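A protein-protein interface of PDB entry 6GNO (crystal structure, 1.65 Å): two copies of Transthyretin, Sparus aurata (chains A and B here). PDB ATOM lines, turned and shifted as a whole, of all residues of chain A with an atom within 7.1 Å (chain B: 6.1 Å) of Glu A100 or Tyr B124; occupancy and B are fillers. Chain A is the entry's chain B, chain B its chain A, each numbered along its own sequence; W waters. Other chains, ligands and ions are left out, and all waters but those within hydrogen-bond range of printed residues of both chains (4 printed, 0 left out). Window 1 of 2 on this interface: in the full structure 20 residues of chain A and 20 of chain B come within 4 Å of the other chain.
The backbone NH of Leu B118 is in hydrogen-bond range of the backbone carbonyl oxygen of Thr B125 (3.0 Å). The backbone NH (N) of Val A79 sits at hydrogen-bond distance from the backbone carbonyl oxygen (O) of Val A101, at 2.8 Å. The side-chain hydroxyl (OH) of Tyr B124 is in hydrogen-bond range of the backbone NH (N) of Glu B100 (3.4 Å).
Glu B100 touches its own counterpart, Glu A100. Tyr B124 touches its own counterpart, Tyr A124. Tyr A124 touches Thr B126, and with the chains exchanged Thr A126 touches Tyr B124. Thr A125 touches its own counterpart, Thr B125.
Printed residues of chain B within 4 Å of Glu A100: Glu B100 (3.6 Å) and Tyr B124 (3.5 Å). Of the printed residues of chain A, Tyr B124 touches Glu A100, Tyr A124, Thr A125 and Thr A126. Of the printed residues of chain B, Val A102 touches His B96 (3.3 Å) and Val B98 (3.9 Å). Of the printed residues of chain A, Ser B123 touches Thr A125 (3.5 Å), Thr A126 (3.2 Å) and Thr A127 (2.8 Å). Of the printed residues of chain B, Thr A125 touches Ser B123 (3.5 Å), Tyr B124 (3.3 Å) and Thr B125 (2.7 Å). Of the printed residues of chain A, Val B102 touches Val A98.
The backbone carbonyl oxygen (O) of Glu A100 is in hydrogen-bond range of the side-chain hydroxyl (OH) of Tyr B124 (3.5 Å). The side-chain hydroxyl (OG) of Ser B123 lies close to the backbone carbonyl oxygen (O) of Thr A126 (3.4 Å). A ring nitrogen (NE2) of His B96 lies within hydrogen-bond range of the side-chain hydroxyl of Thr A126. The side-chain hydroxyl (OG) of Ser B123 sits at hydrogen-bond distance from the side-chain hydroxyl (OG1) of Thr A127, at 2.8 Å. O of Phe B122 sits at hydrogen-bond distance from N of Ala A128 (3.2 Å). The side-chain hydroxyl (OH) of Tyr A124 lies within hydrogen-bond range of the backbone carbonyl oxygen (O) of Glu B100, at 3.5 Å. OG1 of Thr A125 sits at hydrogen-bond distance from OG1 of Thr B125, 2.7 Å away. O of Tyr B124 sits at hydrogen-bond distance from N of Thr A126 (2.9 Å). The backbone NH (N) of Thr B126 sits at hydrogen-bond distance from the backbone carbonyl oxygen (O) of Tyr A124 (2.9 Å).
Of the 18 printed residues of chain B, 9 touch a printed residue of chain A. Hydrophobic or aromatic side chains of chain B that line the printed part of chain A: His B96, Val B102, Phe B122 and Tyr B124. Along chain B the printed residues that touch a printed residue of chain A span positions 96 to 126. Hydrophobic or aromatic side chains of chain A within 4 Å of the printed part of chain B: Val A98, Val A101 and Tyr A124. Among the printed residues, no Asp or Glu carboxylate lies within 4 Å of a Lys or Arg side-chain nitrogen of the other chain.
Water W1 lies within hydrogen-bond range of OH of Tyr B124, O of Glu A100, OH of Tyr A124 and O of Glu B100. Water W3 lies within hydrogen-bond range of the backbone carbonyl oxygen (O) of Val A98 (2.7 Å), the side-chain hydroxyl (OH) of Tyr A124 (2.8 Å), the backbone NH (N) of Val B102 (3.0 Å) and the backbone carbonyl oxygen (O) of Glu B100 (3.4 Å). Water W2 lies within hydrogen-bond range of the side-chain hydroxyl (OH) of Tyr B124 (2.7 Å), the backbone carbonyl oxygen (O) of Val B98 (2.7 Å), the backbone NH (N) of Val A102 (2.8 Å) and the backbone carbonyl oxygen (O) of Glu A100 (3.4 Å). Water W4 bridges N of Glu A100 (2.9 Å) and O of Glu B100 (3.4 Å).
Val A98 touches Val B102 (CG1 to CB, 3.9 Å). Glu A100 touches Glu B100 (OE1 to CG, 3.6 Å). His B96 touches Val A101. His B96 touches Val A102 (CA to O, 3.3 Å). Val A102 touches Val B98. Tyr B124 touches Tyr A124. O of Tyr A124 touches CA of Thr B125, at 3.3 Å. OG of Ser B123 touches CG2 of Thr A125 (3.5 Å). Thr A125 touches Tyr B124 (CA to O, 3.3 Å). Thr A127 touches Phe B122.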
ATOM      1  N   TRP A  49     -13.057  -9.550  32.504  1.00  0.00           N
ATOM      2  CA  TRP A  49     -13.576 -10.779  31.922  1.00  0.00           C
ATOM      3  C   TRP A  49     -12.908 -11.982  32.559  1.00  0.00           C
ATOM      4  O   TRP A  49     -11.687 -12.011  32.731  1.00  0.00           O
ATOM      5  CB  TRP A  49     -13.360 -10.832  30.403  1.00  0.00           C
ATOM      6  CG  TRP A  49     -14.109  -9.778  29.657  1.00  0.00           C
ATOM      7  CD1 TRP A  49     -13.617  -8.593  29.191  1.00  0.00           C
ATOM      8  CD2 TRP A  49     -15.489  -9.809  29.290  1.00  0.00           C
ATOM      9  NE1 TRP A  49     -14.604  -7.885  28.563  1.00  0.00           N
ATOM     10  CE2 TRP A  49     -15.766  -8.608  28.609  1.00  0.00           C
ATOM     11  CE3 TRP A  49     -16.519 -10.736  29.471  1.00  0.00           C
ATOM     12  CZ2 TRP A  49     -17.031  -8.316  28.101  1.00  0.00           C
ATOM     13  CZ3 TRP A  49     -17.775 -10.445  28.969  1.00  0.00           C
ATOM     14  CH2 TRP A  49     -18.022  -9.243  28.302  1.00  0.00           C
ATOM     15  N   ARG A  78     -19.667 -13.133  27.024  1.00  0.00           N
ATOM     16  CA  ARG A  78     -19.030 -12.960  25.728  1.00  0.00           C
ATOM     17  C   ARG A  78     -18.611 -14.323  25.198  1.00  0.00           C
ATOM     18  O   ARG A  78     -17.967 -15.092  25.904  1.00  0.00           O
ATOM     19  CB  ARG A  78     -17.820 -12.039  25.877  1.00  0.00           C
ATOM     20  CG  ARG A  78     -16.921 -11.946  24.708  1.00  0.00           C
ATOM     21  CD  ARG A  78     -15.820 -10.982  25.039  1.00  0.00           C
ATOM     22  NE  ARG A  78     -14.699 -11.601  25.727  1.00  0.00           N
ATOM     23  CZ  ARG A  78     -13.622 -10.924  26.089  1.00  0.00           C
ATOM     24  NH1 ARG A  78     -13.557  -9.620  25.840  1.00  0.00           N
ATOM     25  NH2 ARG A  78     -12.615 -11.533  26.690  1.00  0.00           N
ATOM     26  N   VAL A  79     -18.976 -14.626  23.963  1.00  0.00           N
ATOM     27  CA  VAL A  79     -18.430 -15.777  23.265  1.00  0.00           C
ATOM     28  C   VAL A  79     -17.569 -15.260  22.121  1.00  0.00           C
ATOM     29  O   VAL A  79     -18.064 -14.549  21.229  1.00  0.00           O
ATOM     30  CB  VAL A  79     -19.526 -16.720  22.758  1.00  0.00           C
ATOM     31  CG1 VAL A  79     -18.868 -17.893  22.057  1.00  0.00           C
ATOM     32  CG2 VAL A  79     -20.406 -17.203  23.909  1.00  0.00           C
ATOM     33  N   GLU A  80     -16.280 -15.637  22.139  1.00  0.00           N
ATOM     34  CA  GLU A  80     -15.328 -15.296  21.084  1.00  0.00           C
ATOM     35  C   GLU A  80     -15.146 -16.502  20.174  1.00  0.00           C
ATOM     36  O   GLU A  80     -14.626 -17.528  20.613  1.00  0.00           O
ATOM     37  CB  GLU A  80     -13.954 -14.919  21.633  1.00  0.00           C
ATOM     38  CG  GLU A  80     -13.907 -13.845  22.617  1.00  0.00           C
ATOM     39  CD  GLU A  80     -12.504 -13.762  23.209  1.00  0.00           C
ATOM     40  OE1 GLU A  80     -12.295 -14.216  24.373  1.00  0.00           O
ATOM     41  OE2 GLU A  80     -11.609 -13.288  22.471  1.00  0.00           O
ATOM     42  N   PHE A  81     -15.554 -16.366  18.914  1.00  0.00           N
ATOM     43  CA  PHE A  81     -15.415 -17.412  17.909  1.00  0.00           C
ATOM     44  C   PHE A  81     -14.191 -17.094  17.056  1.00  0.00           C
ATOM     45  O   PHE A  81     -14.076 -15.981  16.524  1.00  0.00           O
ATOM     46  CB  PHE A  81     -16.656 -17.476  17.017  1.00  0.00           C
ATOM     47  CG  PHE A  81     -17.940 -17.784  17.732  1.00  0.00           C
ATOM     48  CD1 PHE A  81     -18.702 -16.776  18.299  1.00  0.00           C
ATOM     49  CD2 PHE A  81     -18.452 -19.068  17.727  1.00  0.00           C
ATOM     50  CE1 PHE A  81     -19.918 -17.069  18.931  1.00  0.00           C
ATOM     51  CE2 PHE A  81     -19.660 -19.367  18.349  1.00  0.00           C
ATOM     52  CZ  PHE A  81     -20.393 -18.357  18.945  1.00  0.00           C
ATOM     53  N   THR A  83     -13.064 -17.119  14.073  1.00  0.00           N
ATOM     54  CA  THR A  83     -13.469 -17.199  12.676  1.00  0.00           C
ATOM     55  C   THR A  83     -12.311 -16.915  11.727  1.00  0.00           C
ATOM     56  O   THR A  83     -12.312 -17.412  10.602  1.00  0.00           O
ATOM     57  CB  THR A  83     -14.640 -16.246  12.415  1.00  0.00           C
ATOM     58  OG1 THR A  83     -14.291 -14.914  12.801  1.00  0.00           O
ATOM     59  CG2 THR A  83     -15.875 -16.691  13.202  1.00  0.00           C
ATOM     60  N   VAL A  98     -11.836 -11.741  14.786  1.00  0.00           N
ATOM     61  CA  VAL A  98     -12.556 -12.629  15.698  1.00  0.00           C
ATOM     62  C   VAL A  98     -14.025 -12.267  15.577  1.00  0.00           C
ATOM     63  O   VAL A  98     -14.367 -11.181  15.109  1.00  0.00           O
ATOM     64  CB  VAL A  98     -12.022 -12.471  17.149  1.00  0.00           C
ATOM     65  CG1 VAL A  98     -12.232 -11.077  17.674  1.00  0.00           C
ATOM     66  CG2 VAL A  98     -12.654 -13.443  18.058  1.00  0.00           C
ATOM     67  N   ALA A  99     -14.899 -13.192  15.931  1.00  0.00           N
ATOM     68  CA  ALA A  99     -16.322 -12.907  15.987  1.00  0.00           C
ATOM     69  C   ALA A  99     -16.717 -12.924  17.460  1.00  0.00           C
ATOM     70  O   ALA A  99     -16.694 -13.979  18.088  1.00  0.00           O
ATOM     71  CB  ALA A  99     -17.099 -13.928  15.158  1.00  0.00           C
ATOM     72  N   GLU A 100     -17.055 -11.759  18.018  1.00  0.00           N
ATOM     73  CA  GLU A 100     -17.418 -11.636  19.430  1.00  0.00           C
ATOM     74  C   GLU A 100     -18.915 -11.438  19.575  1.00  0.00           C
ATOM     75  O   GLU A 100     -19.478 -10.486  19.016  1.00  0.00           O
ATOM     76  CB  GLU A 100     -16.726 -10.455  20.112  1.00  0.00           C
ATOM     77  CG  GLU A 100     -15.235 -10.529  20.256  1.00  0.00           C
ATOM     78  CD  GLU A 100     -14.714  -9.451  21.194  1.00  0.00           C
ATOM     79  OE1 GLU A 100     -15.519  -8.650  21.708  1.00  0.00           O
ATOM     80  OE2 GLU A 100     -13.494  -9.410  21.432  1.00  0.00           O
ATOM     81  N   VAL A 101     -19.552 -12.288  20.373  1.00  0.00           N
ATOM     82  CA  VAL A 101     -20.978 -12.144  20.660  1.00  0.00           C
ATOM     83  C   VAL A 101     -21.116 -11.830  22.139  1.00  0.00           C
ATOM     84  O   VAL A 101     -20.750 -12.646  22.991  1.00  0.00           O
ATOM     85  CB  VAL A 101     -21.765 -13.398  20.250  1.00  0.00           C
ATOM     86  CG1 VAL A 101     -23.266 -13.221  20.518  1.00  0.00           C
ATOM     87  CG2 VAL A 101     -21.528 -13.684  18.784  1.00  0.00           C
ATOM     88  N   VAL A 102     -21.610 -10.630  22.449  1.00  0.00           N
ATOM     89  CA  VAL A 102     -21.657 -10.123  23.814  1.00  0.00           C
ATOM     90  C   VAL A 102     -23.117  -9.908  24.157  1.00  0.00           C
ATOM     91  O   VAL A 102     -23.810  -9.166  23.451  1.00  0.00           O
ATOM     92  CB  VAL A 102     -20.859  -8.814  23.965  1.00  0.00           C
ATOM     93  CG1 VAL A 102     -20.801  -8.365  25.442  1.00  0.00           C
ATOM     94  CG2 VAL A 102     -19.476  -8.984  23.408  1.00  0.00           C
ATOM     95  N   LEU A 117     -24.819 -18.435  14.178  1.00  0.00           N
ATOM     96  CA  LEU A 117     -23.777 -17.638  13.552  1.00  0.00           C
ATOM     97  C   LEU A 117     -23.654 -18.076  12.102  1.00  0.00           C
ATOM     98  O   LEU A 117     -23.459 -19.261  11.827  1.00  0.00           O
ATOM     99  CB  LEU A 117     -22.468 -17.810  14.320  1.00  0.00           C
ATOM    100  CG  LEU A 117     -21.321 -16.874  14.053  1.00  0.00           C
ATOM    101  CD1 LEU A 117     -21.705 -15.449  14.426  1.00  0.00           C
ATOM    102  CD2 LEU A 117     -20.113 -17.396  14.853  1.00  0.00           C
ATOM    103  N   TYR A 124     -20.563 -11.537   8.903  1.00  0.00           N
ATOM    104  CA  TYR A 124     -21.268 -12.570   9.649  1.00  0.00           C
ATOM    105  C   TYR A 124     -22.500 -11.984  10.322  1.00  0.00           C
ATOM    106  O   TYR A 124     -22.610 -10.777  10.576  1.00  0.00           O
ATOM    107  CB  TYR A 124     -20.385 -13.291  10.690  1.00  0.00           C
ATOM    108  CG  TYR A 124     -19.839 -12.460  11.813  1.00  0.00           C
ATOM    109  CD1 TYR A 124     -20.608 -12.135  12.922  1.00  0.00           C
ATOM    110  CD2 TYR A 124     -18.490 -12.078  11.812  1.00  0.00           C
ATOM    111  CE1 TYR A 124     -20.073 -11.388  13.957  1.00  0.00           C
ATOM    112  CE2 TYR A 124     -17.944 -11.337  12.836  1.00  0.00           C
ATOM    113  CZ  TYR A 124     -18.734 -10.994  13.903  1.00  0.00           C
ATOM    114  OH  TYR A 124     -18.191 -10.247  14.908  1.00  0.00           O
ATOM    115  N   THR A 125     -23.436 -12.877  10.582  1.00  0.00           N
ATOM    116  CA  THR A 125     -24.681 -12.564  11.258  1.00  0.00           C
ATOM    117  C   THR A 125     -24.711 -13.349  12.555  1.00  0.00           C
ATOM    118  O   THR A 125     -24.505 -14.562  12.537  1.00  0.00           O
ATOM    119  CB  THR A 125     -25.875 -12.934  10.377  1.00  0.00           C
ATOM    120  OG1 THR A 125     -25.853 -12.137   9.191  1.00  0.00           O
ATOM    121  CG2 THR A 125     -27.198 -12.664  11.100  1.00  0.00           C
ATOM    122  N   THR A 126     -24.967 -12.649  13.670  1.00  0.00           N
ATOM    123  CA  THR A 126     -25.115 -13.242  14.993  1.00  0.00           C
ATOM    124  C   THR A 126     -26.560 -13.063  15.436  1.00  0.00           C
ATOM    125  O   THR A 126     -27.056 -11.926  15.525  1.00  0.00           O
ATOM    126  CB  THR A 126     -24.130 -12.631  16.014  1.00  0.00           C
ATOM    127  OG1 THR A 126     -24.560 -12.904  17.352  1.00  0.00           O
ATOM    128  CG2 THR A 126     -23.984 -11.117  15.863  1.00  0.00           C
ATOM    129  N   THR A 127     -27.242 -14.180  15.654  1.00  0.00           N
ATOM    130  CA  THR A 127     -28.631 -14.204  16.093  1.00  0.00           C
ATOM    131  C   THR A 127     -28.708 -15.052  17.353  1.00  0.00           C
ATOM    132  O   THR A 127     -27.830 -15.868  17.637  1.00  0.00           O
ATOM    133  CB  THR A 127     -29.613 -14.792  15.036  1.00  0.00           C
ATOM    134  OG1 THR A 127     -29.363 -14.267  13.729  1.00  0.00           O
ATOM    135  CG2 THR A 127     -31.038 -14.438  15.385  1.00  0.00           C
ATOM    136  N   ALA A 128     -29.773 -14.886  18.099  1.00  0.00           N
ATOM    137  CA  ALA A 128     -30.009 -15.743  19.258  1.00  0.00           C
ATOM    138  C   ALA A 128     -31.396 -16.362  19.177  1.00  0.00           C
ATOM    139  O   ALA A 128     -32.338 -15.708  18.748  1.00  0.00           O
ATOM    140  CB  ALA A 128     -29.860 -14.947  20.562  1.00  0.00           C
ATOM    141  N   TRP B  49      -6.524  -2.303  25.166  1.00  0.00           N
ATOM    142  CA  TRP B  49      -7.254  -1.522  24.182  1.00  0.00           C
ATOM    143  C   TRP B  49      -7.109  -0.048  24.524  1.00  0.00           C
ATOM    144  O   TRP B  49      -7.369   0.346  25.662  1.00  0.00           O
ATOM    145  CB  TRP B  49      -8.725  -1.931  24.173  1.00  0.00           C
ATOM    146  CG  TRP B  49      -8.942  -3.321  23.676  1.00  0.00           C
ATOM    147  CD1 TRP B  49      -9.202  -4.435  24.427  1.00  0.00           C
ATOM    148  CD2 TRP B  49      -8.899  -3.759  22.315  1.00  0.00           C
ATOM    149  NE1 TRP B  49      -9.323  -5.539  23.615  1.00  0.00           N
ATOM    150  CE2 TRP B  49      -9.136  -5.150  22.313  1.00  0.00           C
ATOM    151  CE3 TRP B  49      -8.686  -3.107  21.092  1.00  0.00           C
ATOM    152  CZ2 TRP B  49      -9.167  -5.897  21.134  1.00  0.00           C
ATOM    153  CZ3 TRP B  49      -8.694  -3.844  19.937  1.00  0.00           C
ATOM    154  CH2 TRP B  49      -8.946  -5.223  19.960  1.00  0.00           C
ATOM    155  N   ARG B  78     -10.933  -2.362  17.323  1.00  0.00           N
ATOM    156  CA  ARG B  78     -12.258  -2.753  17.776  1.00  0.00           C
ATOM    157  C   ARG B  78     -13.171  -1.547  17.660  1.00  0.00           C
ATOM    158  O   ARG B  78     -12.853  -0.469  18.182  1.00  0.00           O
ATOM    159  CB  ARG B  78     -12.231  -3.236  19.223  1.00  0.00           C
ATOM    160  CG  ARG B  78     -13.610  -3.402  19.857  1.00  0.00           C
ATOM    161  CD  ARG B  78     -13.477  -3.829  21.313  1.00  0.00           C
ATOM    162  NE  ARG B  78     -13.148  -2.720  22.204  1.00  0.00           N
ATOM    163  CZ  ARG B  78     -12.865  -2.874  23.494  1.00  0.00           C
ATOM    164  NH1 ARG B  78     -12.863  -4.082  24.048  1.00  0.00           N
ATOM    165  NH2 ARG B  78     -12.578  -1.808  24.233  1.00  0.00           N
ATOM    166  N   THR B  83     -25.580  -0.914  20.772  1.00  0.00           N
ATOM    167  CA  THR B  83     -26.860  -1.274  20.190  1.00  0.00           C
ATOM    168  C   THR B  83     -27.928  -1.471  21.261  1.00  0.00           C
ATOM    169  O   THR B  83     -29.100  -1.264  20.996  1.00  0.00           O
ATOM    170  CB  THR B  83     -26.702  -2.557  19.378  1.00  0.00           C
ATOM    171  OG1 THR B  83     -26.064  -3.536  20.197  1.00  0.00           O
ATOM    172  CG2 THR B  83     -25.820  -2.308  18.168  1.00  0.00           C
ATOM    173  N   HIS B  96     -28.225  -8.443  22.417  1.00  0.00           N
ATOM    174  CA  HIS B  96     -26.809  -8.124  22.571  1.00  0.00           C
ATOM    175  C   HIS B  96     -26.584  -6.909  23.469  1.00  0.00           C
ATOM    176  O   HIS B  96     -27.388  -5.978  23.522  1.00  0.00           O
ATOM    177  CB  HIS B  96     -26.156  -7.850  21.213  1.00  0.00           C
ATOM    178  CG  HIS B  96     -26.268  -8.978  20.231  1.00  0.00           C
ATOM    179  ND1 HIS B  96     -27.294  -9.063  19.312  1.00  0.00           N
ATOM    180  CD2 HIS B  96     -25.448 -10.025  19.975  1.00  0.00           C
ATOM    181  CE1 HIS B  96     -27.118 -10.137  18.557  1.00  0.00           C
ATOM    182  NE2 HIS B  96     -26.004 -10.738  18.939  1.00  0.00           N
ATOM    183  N   VAL B  98     -23.687  -5.107  23.168  1.00  0.00           N
ATOM    184  CA  VAL B  98     -23.045  -4.224  22.207  1.00  0.00           C
ATOM    185  C   VAL B  98     -22.893  -5.028  20.924  1.00  0.00           C
ATOM    186  O   VAL B  98     -23.028  -6.248  20.925  1.00  0.00           O
ATOM    187  CB  VAL B  98     -21.661  -3.727  22.689  1.00  0.00           C
ATOM    188  CG1 VAL B  98     -21.811  -2.808  23.878  1.00  0.00           C
ATOM    189  CG2 VAL B  98     -20.760  -4.926  23.016  1.00  0.00           C
ATOM    190  N   ALA B  99     -22.626  -4.334  19.820  1.00  0.00           N
ATOM    191  CA  ALA B  99     -22.131  -4.968  18.606  1.00  0.00           C
ATOM    192  C   ALA B  99     -20.640  -4.691  18.512  1.00  0.00           C
ATOM    193  O   ALA B  99     -20.212  -3.545  18.668  1.00  0.00           O
ATOM    194  CB  ALA B  99     -22.839  -4.454  17.353  1.00  0.00           C
ATOM    195  N   GLU B 100     -19.858  -5.743  18.289  1.00  0.00           N
ATOM    196  CA  GLU B 100     -18.404  -5.653  18.222  1.00  0.00           C
ATOM    197  C   GLU B 100     -17.911  -5.974  16.821  1.00  0.00           C
ATOM    198  O   GLU B 100     -18.242  -7.025  16.256  1.00  0.00           O
ATOM    199  CB  GLU B 100     -17.751  -6.614  19.210  1.00  0.00           C
ATOM    200  CG  GLU B 100     -18.124  -6.382  20.665  1.00  0.00           C
ATOM    201  CD  GLU B 100     -17.313  -5.283  21.311  1.00  0.00           C
ATOM    202  OE1 GLU B 100     -16.716  -4.480  20.579  1.00  0.00           O
ATOM    203  OE2 GLU B 100     -17.230  -5.253  22.556  1.00  0.00           O
ATOM    204  N   VAL B 101     -17.067  -5.109  16.294  1.00  0.00           N
ATOM    205  CA  VAL B 101     -16.397  -5.359  15.026  1.00  0.00           C
ATOM    206  C   VAL B 101     -14.896  -5.219  15.247  1.00  0.00           C
ATOM    207  O   VAL B 101     -14.397  -4.113  15.519  1.00  0.00           O
ATOM    208  CB  VAL B 101     -16.900  -4.410  13.932  1.00  0.00           C
ATOM    209  CG1 VAL B 101     -16.196  -4.675  12.636  1.00  0.00           C
ATOM    210  CG2 VAL B 101     -18.403  -4.593  13.762  1.00  0.00           C
ATOM    211  N   VAL B 102     -14.180  -6.335  15.135  1.00  0.00           N
ATOM    212  CA  VAL B 102     -12.751  -6.404  15.408  1.00  0.00           C
ATOM    213  C   VAL B 102     -12.034  -6.849  14.146  1.00  0.00           C
ATOM    214  O   VAL B 102     -12.362  -7.899  13.584  1.00  0.00           O
ATOM    215  CB  VAL B 102     -12.441  -7.386  16.552  1.00  0.00           C
ATOM    216  CG1 VAL B 102     -10.953  -7.346  16.888  1.00  0.00           C
ATOM    217  CG2 VAL B 102     -13.242  -7.022  17.770  1.00  0.00           C
ATOM    218  N   LEU B 117     -23.511  -2.290   9.315  1.00  0.00           N
ATOM    219  CA  LEU B 117     -24.129  -2.965  10.436  1.00  0.00           C
ATOM    220  C   LEU B 117     -25.631  -2.895  10.251  1.00  0.00           C
ATOM    221  O   LEU B 117     -26.187  -1.818  10.026  1.00  0.00           O
ATOM    222  CB  LEU B 117     -23.691  -2.317  11.751  1.00  0.00           C
ATOM    223  CG  LEU B 117     -24.020  -2.976  13.076  1.00  0.00           C
ATOM    224  CD1 LEU B 117     -23.286  -4.295  13.295  1.00  0.00           C
ATOM    225  CD2 LEU B 117     -23.638  -1.951  14.159  1.00  0.00           C
ATOM    226  N   LEU B 118     -26.259  -4.057  10.284  1.00  0.00           N
ATOM    227  CA  LEU B 118     -27.700  -4.213  10.146  1.00  0.00           C
ATOM    228  C   LEU B 118     -28.238  -4.715  11.479  1.00  0.00           C
ATOM    229  O   LEU B 118     -27.859  -5.803  11.918  1.00  0.00           O
ATOM    230  CB  LEU B 118     -28.012  -5.222   9.055  1.00  0.00           C
ATOM    231  CG  LEU B 118     -29.476  -5.529   8.862  1.00  0.00           C
ATOM    232  CD1 LEU B 118     -30.211  -4.235   8.383  1.00  0.00           C
ATOM    233  CD2 LEU B 118     -29.671  -6.710   7.901  1.00  0.00           C
ATOM    234  N   LEU B 119     -29.161  -3.968  12.081  1.00  0.00           N
ATOM    235  CA  LEU B 119     -29.607  -4.242  13.443  1.00  0.00           C
ATOM    236  C   LEU B 119     -31.071  -4.682  13.499  1.00  0.00           C
ATOM    237  O   LEU B 119     -31.948  -4.035  12.921  1.00  0.00           O
ATOM    238  CB  LEU B 119     -29.458  -3.005  14.331  1.00  0.00           C
ATOM    239  CG  LEU B 119     -28.124  -2.318  14.375  1.00  0.00           C
ATOM    240  CD1 LEU B 119     -28.248  -1.071  15.271  1.00  0.00           C
ATOM    241  CD2 LEU B 119     -27.085  -3.272  14.882  1.00  0.00           C
ATOM    242  N   SER B 120     -31.323  -5.743  14.258  1.00  0.00           N
ATOM    243  CA  SER B 120     -32.622  -6.143  14.769  1.00  0.00           C
ATOM    244  C   SER B 120     -32.463  -6.424  16.258  1.00  0.00           C
ATOM    245  O   SER B 120     -31.350  -6.663  16.734  1.00  0.00           O
ATOM    246  CB  SER B 120     -33.138  -7.401  14.065  1.00  0.00           C
ATOM    247  OG  SER B 120     -33.118  -7.264  12.660  1.00  0.00           O
ATOM    248  N   PHE B 122     -32.825  -9.048  18.135  1.00  0.00           N
ATOM    249  CA  PHE B 122     -32.124 -10.284  18.468  1.00  0.00           C
ATOM    250  C   PHE B 122     -31.143 -10.757  17.393  1.00  0.00           C
ATOM    251  O   PHE B 122     -30.795 -11.949  17.362  1.00  0.00           O
ATOM    252  CB  PHE B 122     -33.144 -11.378  18.774  1.00  0.00           C
ATOM    253  CG  PHE B 122     -33.500 -11.437  20.217  1.00  0.00           C
ATOM    254  CD1 PHE B 122     -34.232 -10.438  20.804  1.00  0.00           C
ATOM    255  CD2 PHE B 122     -33.070 -12.484  20.994  1.00  0.00           C
ATOM    256  CE1 PHE B 122     -34.535 -10.503  22.147  1.00  0.00           C
ATOM    257  CE2 PHE B 122     -33.372 -12.551  22.326  1.00  0.00           C
ATOM    258  CZ  PHE B 122     -34.101 -11.575  22.900  1.00  0.00           C
ATOM    259  N   SER B 123     -30.655  -9.853  16.543  1.00  0.00           N
ATOM    260  CA  SER B 123     -29.746 -10.256  15.480  1.00  0.00           C
ATOM    261  C   SER B 123     -29.030  -9.029  14.950  1.00  0.00           C
ATOM    262  O   SER B 123     -29.635  -7.970  14.846  1.00  0.00           O
ATOM    263  CB  SER B 123     -30.506 -10.930  14.332  1.00  0.00           C
ATOM    264  OG  SER B 123     -29.624 -11.482  13.384  1.00  0.00           O
ATOM    265  N   TYR B 124     -27.747  -9.162  14.614  1.00  0.00           N
ATOM    266  CA  TYR B 124     -27.142  -8.164  13.738  1.00  0.00           C
ATOM    267  C   TYR B 124     -26.189  -8.824  12.756  1.00  0.00           C
ATOM    268  O   TYR B 124     -25.699  -9.930  12.960  1.00  0.00           O
ATOM    269  CB  TYR B 124     -26.409  -7.033  14.497  1.00  0.00           C
ATOM    270  CG  TYR B 124     -25.206  -7.432  15.335  1.00  0.00           C
ATOM    271  CD1 TYR B 124     -23.955  -7.572  14.758  1.00  0.00           C
ATOM    272  CD2 TYR B 124     -25.310  -7.596  16.727  1.00  0.00           C
ATOM    273  CE1 TYR B 124     -22.853  -7.915  15.508  1.00  0.00           C
ATOM    274  CE2 TYR B 124     -24.208  -7.924  17.484  1.00  0.00           C
ATOM    275  CZ  TYR B 124     -22.978  -8.066  16.881  1.00  0.00           C
ATOM    276  OH  TYR B 124     -21.891  -8.388  17.663  1.00  0.00           O
ATOM    277  N   THR B 125     -25.969  -8.122  11.658  1.00  0.00           N
ATOM    278  CA  THR B 125     -25.019  -8.524  10.629  1.00  0.00           C
ATOM    279  C   THR B 125     -23.939  -7.460  10.551  1.00  0.00           C
ATOM    280  O   THR B 125     -24.254  -6.279  10.482  1.00  0.00           O
ATOM    281  CB  THR B 125     -25.703  -8.658   9.271  1.00  0.00           C
ATOM    282  OG1 THR B 125     -26.763  -9.631   9.330  1.00  0.00           O
ATOM    283  CG2 THR B 125     -24.691  -9.070   8.193  1.00  0.00           C
ATOM    284  N   THR B 126     -22.677  -7.880  10.543  1.00  0.00           N
ATOM    285  CA  THR B 126     -21.533  -6.980  10.402  1.00  0.00           C
ATOM    286  C   THR B 126     -20.808  -7.357   9.122  1.00  0.00           C
ATOM    287  O   THR B 126     -20.280  -8.467   9.011  1.00  0.00           O
ATOM    288  CB  THR B 126     -20.570  -7.048  11.604  1.00  0.00           C
ATOM    289  OG1 THR B 126     -19.277  -6.515  11.242  1.00  0.00           O
ATOM    290  CG2 THR B 126     -20.379  -8.460  12.081  1.00  0.00           C
HETATM  291  O   HOH W   1     -19.663  -9.215  16.785  1.00  0.00           O
HETATM  292  O   HOH W   2     -22.073  -8.755  20.362  1.00  0.00           O
HETATM  293  O   HOH W   3     -15.727  -8.859  14.991  1.00  0.00           O
HETATM  294  O   HOH W   4     -15.992  -9.111  17.663  1.00  0.00           O
